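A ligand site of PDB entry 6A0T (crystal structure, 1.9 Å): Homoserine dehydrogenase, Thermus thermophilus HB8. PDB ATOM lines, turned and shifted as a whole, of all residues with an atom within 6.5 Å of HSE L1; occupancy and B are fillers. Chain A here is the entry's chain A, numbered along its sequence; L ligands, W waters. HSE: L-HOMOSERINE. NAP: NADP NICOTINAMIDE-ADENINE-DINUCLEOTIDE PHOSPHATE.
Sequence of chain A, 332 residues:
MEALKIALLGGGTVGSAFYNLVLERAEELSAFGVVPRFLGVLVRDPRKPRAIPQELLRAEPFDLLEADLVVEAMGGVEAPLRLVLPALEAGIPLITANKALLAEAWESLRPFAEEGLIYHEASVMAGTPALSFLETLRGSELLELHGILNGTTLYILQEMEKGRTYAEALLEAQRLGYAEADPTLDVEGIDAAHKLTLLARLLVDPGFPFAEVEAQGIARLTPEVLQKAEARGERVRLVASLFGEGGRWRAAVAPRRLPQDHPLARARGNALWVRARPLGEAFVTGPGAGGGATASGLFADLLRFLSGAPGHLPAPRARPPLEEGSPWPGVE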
ATOM      1  N   ALA A  97      29.994  -6.933 -16.119  1.00  0.00           N
ATOM      2  CA  ALA A  97      28.908  -6.909 -17.120  1.00  0.00           C
ATOM      3  C   ALA A  97      28.295  -8.247 -17.433  1.00  0.00           C
ATOM      4  O   ALA A  97      27.477  -8.400 -18.360  1.00  0.00           O
ATOM      5  CB  ALA A  97      29.422  -6.282 -18.410  1.00  0.00           C
ATOM      6  N   LYS A  99      25.967 -11.105 -16.924  1.00  0.00           N
ATOM      7  CA  LYS A  99      24.680 -11.616 -16.435  1.00  0.00           C
ATOM      8  C   LYS A  99      24.718 -13.154 -16.236  1.00  0.00           C
ATOM      9  O   LYS A  99      24.135 -13.662 -15.269  1.00  0.00           O
ATOM     10  CB  LYS A  99      23.491 -11.226 -17.305  1.00  0.00           C
ATOM     11  N   ALA A 122      26.055  -2.804 -15.706  1.00  0.00           N
ATOM     12  CA  ALA A 122      26.231  -3.085 -17.133  1.00  0.00           C
ATOM     13  C   ALA A 122      25.733  -4.462 -17.540  1.00  0.00           C
ATOM     14  O   ALA A 122      25.703  -4.788 -18.709  1.00  0.00           O
ATOM     15  CB  ALA A 122      27.717  -2.968 -17.494  1.00  0.00           C
ATOM     16  N   SER A 123      25.408  -5.335 -16.553  1.00  0.00           N
ATOM     17  CA  SER A 123      24.881  -6.712 -16.849  1.00  0.00           C
ATOM     18  C   SER A 123      23.432  -6.738 -17.310  1.00  0.00           C
ATOM     19  O   SER A 123      22.961  -7.757 -17.750  1.00  0.00           O
ATOM     20  CB  SER A 123      25.061  -7.564 -15.604  1.00  0.00           C
ATOM     21  OG  SER A 123      24.104  -7.266 -14.571  1.00  0.00           O
ATOM     22  N   VAL A 124      22.687  -5.611 -17.168  1.00  0.00           N
ATOM     23  CA  VAL A 124      21.351  -5.546 -17.677  1.00  0.00           C
ATOM     24  C   VAL A 124      21.096  -4.228 -18.406  1.00  0.00           C
ATOM     25  O   VAL A 124      21.215  -3.151 -17.775  1.00  0.00           O
ATOM     26  CB  VAL A 124      20.271  -5.677 -16.534  1.00  0.00           C
ATOM     27  CG1 VAL A 124      18.874  -5.572 -17.142  1.00  0.00           C
ATOM     28  CG2 VAL A 124      20.439  -6.944 -15.723  1.00  0.00           C
ATOM     29  N   MET A 125      20.791  -4.287 -19.680  1.00  0.00           N
ATOM     30  CA  MET A 125      20.647  -3.142 -20.529  1.00  0.00           C
ATOM     31  C   MET A 125      21.836  -2.213 -20.603  1.00  0.00           C
ATOM     32  O   MET A 125      21.683  -0.977 -20.623  1.00  0.00           O
ATOM     33  CB  MET A 125      19.327  -2.350 -20.147  1.00  0.00           C
ATOM     34  CG  MET A 125      18.137  -3.185 -20.459  1.00  0.00           C
ATOM     35  SD  MET A 125      16.540  -2.584 -19.761  1.00  0.00           S
ATOM     36  CE  MET A 125      16.469  -0.941 -20.335  1.00  0.00           C
ATOM     37  N   ALA A 126      23.022  -2.791 -20.462  1.00  0.00           N
ATOM     38  CA  ALA A 126      24.279  -2.057 -20.710  1.00  0.00           C
ATOM     39  C   ALA A 126      24.261  -0.814 -19.806  1.00  0.00           C
ATOM     40  O   ALA A 126      23.905  -0.947 -18.610  1.00  0.00           O
ATOM     41  CB  ALA A 126      24.458  -1.693 -22.164  1.00  0.00           C
ATOM     42  N   LEU A 149      14.815  -7.194 -22.710  1.00  0.00           N
ATOM     43  CA  LEU A 149      16.135  -7.168 -22.133  1.00  0.00           C
ATOM     44  C   LEU A 149      17.295  -7.515 -23.116  1.00  0.00           C
ATOM     45  O   LEU A 149      18.438  -7.205 -22.834  1.00  0.00           O
ATOM     46  CB  LEU A 149      16.233  -8.016 -20.897  1.00  0.00           C
ATOM     47  CG  LEU A 149      15.142  -7.758 -19.813  1.00  0.00           C
ATOM     48  CD1 LEU A 149      15.336  -8.677 -18.651  1.00  0.00           C
ATOM     49  CD2 LEU A 149      15.159  -6.270 -19.366  1.00  0.00           C
ATOM     50  N   ASN A 150      16.958  -8.242 -24.209  1.00  0.00           N
ATOM     51  CA  ASN A 150      17.991  -8.730 -25.103  1.00  0.00           C
ATOM     52  C   ASN A 150      18.063  -7.759 -26.239  1.00  0.00           C
ATOM     53  O   ASN A 150      17.110  -7.559 -26.981  1.00  0.00           O
ATOM     54  CB  ASN A 150      17.688 -10.154 -25.496  1.00  0.00           C
ATOM     55  CG  ASN A 150      18.795 -10.779 -26.379  1.00  0.00           C
ATOM     56  OD1 ASN A 150      18.702 -10.794 -27.604  1.00  0.00           O
ATOM     57  ND2 ASN A 150      19.908 -11.155 -25.716  1.00  0.00           N
ATOM     58  N   GLY A 151      19.227  -7.161 -26.394  1.00  0.00           N
ATOM     59  CA  GLY A 151      19.514  -6.223 -27.457  1.00  0.00           C
ATOM     60  C   GLY A 151      19.486  -6.813 -28.863  1.00  0.00           C
ATOM     61  O   GLY A 151      18.959  -6.250 -29.818  1.00  0.00           O
ATOM     62  N   THR A 152      20.156  -7.967 -28.970  1.00  0.00           N
ATOM     63  CA  THR A 152      20.269  -8.606 -30.289  1.00  0.00           C
ATOM     64  C   THR A 152      18.914  -8.990 -30.868  1.00  0.00           C
ATOM     65  O   THR A 152      18.660  -8.694 -32.052  1.00  0.00           O
ATOM     66  CB  THR A 152      21.167  -9.848 -30.064  1.00  0.00           C
ATOM     67  OG1 THR A 152      22.495  -9.437 -29.730  1.00  0.00           O
ATOM     68  CG2 THR A 152      21.305 -10.762 -31.304  1.00  0.00           C
ATOM     69  N   THR A 153      18.069  -9.633 -30.060  1.00  0.00           N
ATOM     70  CA  THR A 153      16.755 -10.071 -30.492  1.00  0.00           C
ATOM     71  C   THR A 153      15.816  -8.898 -30.848  1.00  0.00           C
ATOM     72  O   THR A 153      15.101  -8.917 -31.845  1.00  0.00           O
ATOM     73  CB  THR A 153      16.157 -11.011 -29.489  1.00  0.00           C
ATOM     74  OG1 THR A 153      16.923 -12.259 -29.520  1.00  0.00           O
ATOM     75  CG2 THR A 153      14.721 -11.391 -29.971  1.00  0.00           C
ATOM     76  N   GLY A 177      28.407  -5.555 -32.500  1.00  0.00           N
ATOM     77  CA  GLY A 177      29.016  -6.021 -31.297  1.00  0.00           C
ATOM     78  C   GLY A 177      27.982  -6.430 -30.272  1.00  0.00           C
ATOM     79  O   GLY A 177      28.306  -6.504 -29.092  1.00  0.00           O
ATOM     80  N   TYR A 178      26.749  -6.660 -30.678  1.00  0.00           N
ATOM     81  CA  TYR A 178      25.667  -6.908 -29.683  1.00  0.00           C
ATOM     82  C   TYR A 178      25.610  -8.346 -29.161  1.00  0.00           C
ATOM     83  O   TYR A 178      25.109  -8.593 -28.085  1.00  0.00           O
ATOM     84  CB  TYR A 178      24.279  -6.604 -30.230  1.00  0.00           C
ATOM     85  CG  TYR A 178      24.043  -5.207 -30.688  1.00  0.00           C
ATOM     86  CD1 TYR A 178      24.832  -4.117 -30.252  1.00  0.00           C
ATOM     87  CD2 TYR A 178      22.994  -4.931 -31.534  1.00  0.00           C
ATOM     88  CE1 TYR A 178      24.536  -2.797 -30.637  1.00  0.00           C
ATOM     89  CE2 TYR A 178      22.764  -3.652 -31.982  1.00  0.00           C
ATOM     90  CZ  TYR A 178      23.565  -2.605 -31.537  1.00  0.00           C
ATOM     91  OH  TYR A 178      23.271  -1.361 -31.991  1.00  0.00           O
ATOM     92  N   ALA A 179      26.010  -9.347 -29.996  1.00  0.00           N
ATOM     93  CA  ALA A 179      25.606 -10.746 -29.717  1.00  0.00           C
ATOM     94  C   ALA A 179      26.542 -11.448 -28.810  1.00  0.00           C
ATOM     95  O   ALA A 179      27.732 -11.141 -28.808  1.00  0.00           O
ATOM     96  CB  ALA A 179      25.560 -11.514 -31.057  1.00  0.00           C
ATOM     97  N   GLU A 180      26.042 -12.424 -28.081  1.00  0.00           N
ATOM     98  CA  GLU A 180      26.936 -13.335 -27.408  1.00  0.00           C
ATOM     99  C   GLU A 180      27.786 -14.154 -28.399  1.00  0.00           C
ATOM    100  O   GLU A 180      27.420 -14.231 -29.559  1.00  0.00           O
ATOM    101  CB  GLU A 180      26.114 -14.270 -26.535  1.00  0.00           C
ATOM    102  CG  GLU A 180      25.284 -13.602 -25.440  1.00  0.00           C
ATOM    103  CD  GLU A 180      26.162 -12.738 -24.578  1.00  0.00           C
ATOM    104  OE1 GLU A 180      25.935 -11.494 -24.641  1.00  0.00           O
ATOM    105  OE2 GLU A 180      27.038 -13.230 -23.888  1.00  0.00           O
ATOM    106  N   ASP A 186      21.189 -15.463 -27.359  1.00  0.00           N
ATOM    107  CA  ASP A 186      20.308 -14.335 -27.622  1.00  0.00           C
ATOM    108  C   ASP A 186      18.930 -14.773 -28.125  1.00  0.00           C
ATOM    109  O   ASP A 186      17.871 -14.469 -27.493  1.00  0.00           O
ATOM    110  CB  ASP A 186      20.954 -13.357 -28.585  1.00  0.00           C
ATOM    111  CG  ASP A 186      22.310 -12.821 -28.030  1.00  0.00           C
ATOM    112  OD1 ASP A 186      22.236 -12.213 -26.927  1.00  0.00           O
ATOM    113  OD2 ASP A 186      23.377 -13.015 -28.620  1.00  0.00           O
ATOM    114  N   ASP A 191      19.942 -15.375 -22.590  1.00  0.00           N
ATOM    115  CA  ASP A 191      20.521 -14.117 -22.094  1.00  0.00           C
ATOM    116  C   ASP A 191      19.433 -13.268 -21.363  1.00  0.00           C
ATOM    117  O   ASP A 191      19.668 -12.792 -20.254  1.00  0.00           O
ATOM    118  CB  ASP A 191      21.200 -13.380 -23.220  1.00  0.00           C
ATOM    119  CG  ASP A 191      21.693 -11.960 -22.772  1.00  0.00           C
ATOM    120  OD1 ASP A 191      20.907 -11.038 -23.070  1.00  0.00           O
ATOM    121  OD2 ASP A 191      22.746 -11.945 -22.102  1.00  0.00           O
ATOM    122  N   LYS A 195      19.199 -12.232 -17.292  1.00  0.00           N
ATOM    123  CA  LYS A 195      18.977 -10.806 -16.825  1.00  0.00           C
ATOM    124  C   LYS A 195      17.699 -10.773 -15.962  1.00  0.00           C
ATOM    125  O   LYS A 195      17.663 -10.148 -14.919  1.00  0.00           O
ATOM    126  CB  LYS A 195      18.907  -9.910 -18.003  1.00  0.00           C
ATOM    127  CG  LYS A 195      20.250  -9.691 -18.686  1.00  0.00           C
ATOM    128  CD  LYS A 195      20.090  -9.072 -20.052  1.00  0.00           C
ATOM    129  CE  LYS A 195      21.494  -8.863 -20.616  1.00  0.00           C
ATOM    130  NZ  LYS A 195      21.363  -8.619 -22.063  1.00  0.00           N
ATOM    131  N   ASN A 270      16.248  -1.063 -25.709  1.00  0.00           N
ATOM    132  CA  ASN A 270      15.751  -2.022 -24.752  1.00  0.00           C
ATOM    133  C   ASN A 270      14.944  -1.246 -23.650  1.00  0.00           C
ATOM    134  O   ASN A 270      15.010   0.027 -23.634  1.00  0.00           O
ATOM    135  CB  ASN A 270      16.840  -2.775 -24.113  1.00  0.00           C
ATOM    136  CG  ASN A 270      17.414  -3.797 -25.128  1.00  0.00           C
ATOM    137  OD1 ASN A 270      18.327  -3.435 -25.916  1.00  0.00           O
ATOM    138  ND2 ASN A 270      16.725  -4.898 -25.304  1.00  0.00           N
ATOM    139  N   GLY A 288      20.769  -1.295 -25.154  1.00  0.00           N
ATOM    140  CA  GLY A 288      20.993  -2.448 -24.318  1.00  0.00           C
ATOM    141  C   GLY A 288      22.145  -3.356 -24.657  1.00  0.00           C
ATOM    142  O   GLY A 288      22.353  -4.343 -23.940  1.00  0.00           O
ATOM    143  N   ALA A 289      22.954  -2.906 -25.607  1.00  0.00           N
ATOM    144  CA  ALA A 289      24.124  -3.658 -25.969  1.00  0.00           C
ATOM    145  C   ALA A 289      25.046  -2.724 -26.725  1.00  0.00           C
ATOM    146  O   ALA A 289      24.656  -1.609 -27.129  1.00  0.00           O
ATOM    147  CB  ALA A 289      23.678  -4.805 -26.859  1.00  0.00           C
ATOM    148  N   GLY A 290      26.268  -3.215 -26.973  1.00  0.00           N
ATOM    149  CA  GLY A 290      27.250  -2.397 -27.671  1.00  0.00           C
ATOM    150  C   GLY A 290      28.396  -2.010 -26.772  1.00  0.00           C
ATOM    151  O   GLY A 290      28.202  -1.885 -25.564  1.00  0.00           O
ATOM    152  N   THR A 294      28.004  -0.336 -22.993  1.00  0.00           N
ATOM    153  CA  THR A 294      28.319  -1.131 -21.892  1.00  0.00           C
ATOM    154  C   THR A 294      29.419  -0.501 -21.052  1.00  0.00           C
ATOM    155  O   THR A 294      29.443  -0.509 -19.798  1.00  0.00           O
ATOM    156  CB  THR A 294      28.630  -2.590 -22.321  1.00  0.00           C
ATOM    157  OG1 THR A 294      27.601  -2.998 -23.179  1.00  0.00           O
ATOM    158  CG2 THR A 294      28.833  -3.470 -21.137  1.00  0.00           C
HETATM  159  N   HSE L   1      24.006 -10.291 -26.137  1.00  0.00           N
HETATM  160  CA  HSE L   1      23.462  -9.252 -25.219  1.00  0.00           C
HETATM  161  C   HSE L   1      22.206  -8.697 -25.800  1.00  0.00           C
HETATM  162  C3  HSE L   1      24.488  -8.147 -25.065  1.00  0.00           C
HETATM  163  O   HSE L   1      21.938  -8.774 -27.056  1.00  0.00           O
HETATM  164  OXT HSE L   1      21.353  -8.095 -25.076  1.00  0.00           O
HETATM  165  C4  HSE L   1      24.011  -7.108 -23.997  1.00  0.00           C
HETATM  166  O3  HSE L   1      23.861  -7.583 -22.645  1.00  0.00           O
HETATM  167  PA  NAP L   2      34.146 -10.556 -26.467  1.00  0.00           P
HETATM  168  O1A NAP L   2      34.134 -11.986 -26.944  1.00  0.00           O
HETATM  169  O2A NAP L   2      34.302  -9.536 -27.404  1.00  0.00           O
HETATM  170  O5B NAP L   2      35.333 -10.452 -25.451  1.00  0.00           O
HETATM  171  C5B NAP L   2      35.681 -11.441 -24.478  1.00  0.00           C
HETATM  172  C4B NAP L   2      37.076 -11.141 -23.985  1.00  0.00           C
HETATM  173  O4B NAP L   2      37.463 -12.019 -23.003  1.00  0.00           O
HETATM  174  C3B NAP L   2      38.152 -11.179 -25.104  1.00  0.00           C
HETATM  175  O3B NAP L   2      39.196 -10.230 -24.760  1.00  0.00           O
HETATM  176  C2B NAP L   2      38.656 -12.650 -24.979  1.00  0.00           C
HETATM  177  O2B NAP L   2      40.019 -12.809 -25.348  1.00  0.00           O
HETATM  178  C1B NAP L   2      38.598 -12.806 -23.482  1.00  0.00           C
HETATM  179  N9A NAP L   2      38.437 -14.179 -22.973  1.00  0.00           N
HETATM  180  C8A NAP L   2      37.348 -14.973 -23.182  1.00  0.00           C
HETATM  181  N7A NAP L   2      37.454 -16.171 -22.571  1.00  0.00           N
HETATM  182  C5A NAP L   2      38.663 -16.078 -21.936  1.00  0.00           C
HETATM  183  C6A NAP L   2      39.377 -16.992 -21.105  1.00  0.00           C
HETATM  184  N6A NAP L   2      38.849 -18.233 -20.849  1.00  0.00           N
HETATM  185  N1A NAP L   2      40.535 -16.643 -20.616  1.00  0.00           N
HETATM  186  C2A NAP L   2      41.087 -15.400 -20.833  1.00  0.00           C
HETATM  187  N3A NAP L   2      40.498 -14.485 -21.617  1.00  0.00           N
HETATM  188  C4A NAP L   2      39.298 -14.797 -22.160  1.00  0.00           C
HETATM  189  O3  NAP L   2      32.864 -10.551 -25.583  1.00  0.00           O
HETATM  190  PN  NAP L   2      32.070  -9.127 -25.146  1.00  0.00           P
HETATM  191  O1N NAP L   2      33.074  -8.135 -24.821  1.00  0.00           O
HETATM  192  O2N NAP L   2      31.067  -8.853 -26.151  1.00  0.00           O
HETATM  193  O5D NAP L   2      31.281  -9.616 -23.859  1.00  0.00           O
HETATM  194  C5D NAP L   2      31.965  -9.808 -22.619  1.00  0.00           C
HETATM  195  C4D NAP L   2      31.013 -10.009 -21.461  1.00  0.00           C
HETATM  196  O4D NAP L   2      30.088  -8.884 -21.402  1.00  0.00           O
HETATM  197  C3D NAP L   2      30.077 -11.248 -21.710  1.00  0.00           C
HETATM  198  O3D NAP L   2      29.876 -11.760 -20.384  1.00  0.00           O
HETATM  199  C2D NAP L   2      28.811 -10.708 -22.342  1.00  0.00           C
HETATM  200  O2D NAP L   2      27.665 -11.433 -21.976  1.00  0.00           O
HETATM  201  C1D NAP L   2      28.744  -9.386 -21.544  1.00  0.00           C
HETATM  202  N1N NAP L   2      28.072  -8.280 -22.169  1.00  0.00           N
HETATM  203  C2N NAP L   2      28.192  -7.958 -23.493  1.00  0.00           C
HETATM  204  C3N NAP L   2      27.656  -6.835 -24.033  1.00  0.00           C
HETATM  205  C7N NAP L   2      27.709  -6.495 -25.478  1.00  0.00           C
HETATM  206  O7N NAP L   2      26.918  -5.696 -25.931  1.00  0.00           O
HETATM  207  N7N NAP L   2      28.612  -7.100 -26.283  1.00  0.00           N
HETATM  208  C4N NAP L   2      26.965  -5.934 -23.177  1.00  0.00           C
HETATM  209  C5N NAP L   2      26.845  -6.256 -21.853  1.00  0.00           C
HETATM  210  C6N NAP L   2      27.406  -7.413 -21.331  1.00  0.00           C
HETATM  211  P2B NAP L   2      40.362 -12.540 -26.939  1.00  0.00           P
HETATM  212  O1X NAP L   2      40.018 -11.152 -27.301  1.00  0.00           O
HETATM  213  O2X NAP L   2      41.834 -12.759 -26.833  1.00  0.00           O
HETATM  214  O3X NAP L   2      39.640 -13.619 -27.595  1.00  0.00           O
HETATM  215  O   HOH W   1      24.808 -10.047 -22.135  1.00  0.00           O
HETATM  216  O   HOH W   2      23.603  -5.643 -20.536  1.00  0.00           O
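N of Glu 180 sits at hydrogen-bond distance from OD2 of Asp 186 (2.8 Å). The side-chain amide nitrogen (ND2) of Asn 150 is in hydrogen-bond range of the side-chain carboxylate (OD1) of Asp 186 (2.8 Å). O of Asp 186 sits at hydrogen-bond distance from OG1 of Thr 153, 3.1 Å away. N of Thr 152 sits close to OD1 of Asn 150 (3.5 Å). The backbone carbonyl oxygen (O) of Leu 149 is in hydrogen-bond range of the side-chain amino group (NZ) of Lys 195, 3.3 Å away. ND2 of Asn 150 lies within hydrogen-bond range of OD1 of Asp 191, 2.8 Å away. OD1 of Asn 150 lies within hydrogen-bond range of N of Thr 153, 2.8 Å away. The side-chain amide nitrogen (ND2) of Asn 270 is in hydrogen-bond range of the backbone carbonyl oxygen (O) of Asn 150 (3.2 Å).
Water W1 lies within hydrogen-bond range of an oxygen (O3) of HSE L1 (2.7 Å), the side-chain carboxylate of Asp 191 (2.8 Å), the side-chain carboxylate of Glu 180 (3.1 Å) and an oxygen (O2D) of NAP L2 (3.2 Å).
Leu 149 touches HSE L1 (O to OXT, 3.8 Å). Ala 179 touches HSE L1. Asp 191 touches HSE L1 (OD1 to OXT, 3.6 Å). O of Gly 288 touches C4 of HSE L1, at 3.2 Å. CB of Ala 289 touches C4 of HSE L1, 3.7 Å away. 12 residues have an atom within 4 Å of HSE L1: Leu 149, Asn 150, Gly 151, Thr 152, Tyr 178, Ala 179, Glu 180, Asp 186, Asp 191, Lys 195, Gly 288 and Ala 289. The nearest printed residue that does not touch HSE L1 is Thr 153 (5.0 Å).
An oxygen (OXT) of HSE L1 is in hydrogen-bond range of the backbone NH (N) of Gly 151. A nitrogen (N) of HSE L1 lies within salt-bridge range of the side-chain carboxylate (OE1) of Glu 180 (2.7 Å). The side-chain carboxylate of Asp 186 is in salt-bridge range of a nitrogen (N) of HSE L1 (2.7 Å). The backbone NH (N) of Thr 152 sits at hydrogen-bond distance from an oxygen (O) of HSE L1 (2.7 Å). An oxygen (O) of HSE L1 lies within hydrogen-bond range of the side-chain hydroxyl of Thr 152. NZ of Lys 195 lies within salt-bridge range of OXT of HSE L1 (3.1 Å). The backbone carbonyl oxygen of Tyr 178 sits at hydrogen-bond distance from a nitrogen (N) of HSE L1 (2.8 Å). An oxygen (O) of HSE L1 lies close to the side-chain amide nitrogen (ND2) of Asn 150. OE2 of Glu 180 lies within hydrogen-bond range of O2D of NAP L2, at 2.7 Å. An oxygen (O7N) of NAP L2 sits at hydrogen-bond distance from the backbone NH of Gly 290. The backbone carbonyl oxygen (O) of Gly 177 is in hydrogen-bond range of a nitrogen (N7N) of NAP L2 (2.9 Å).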
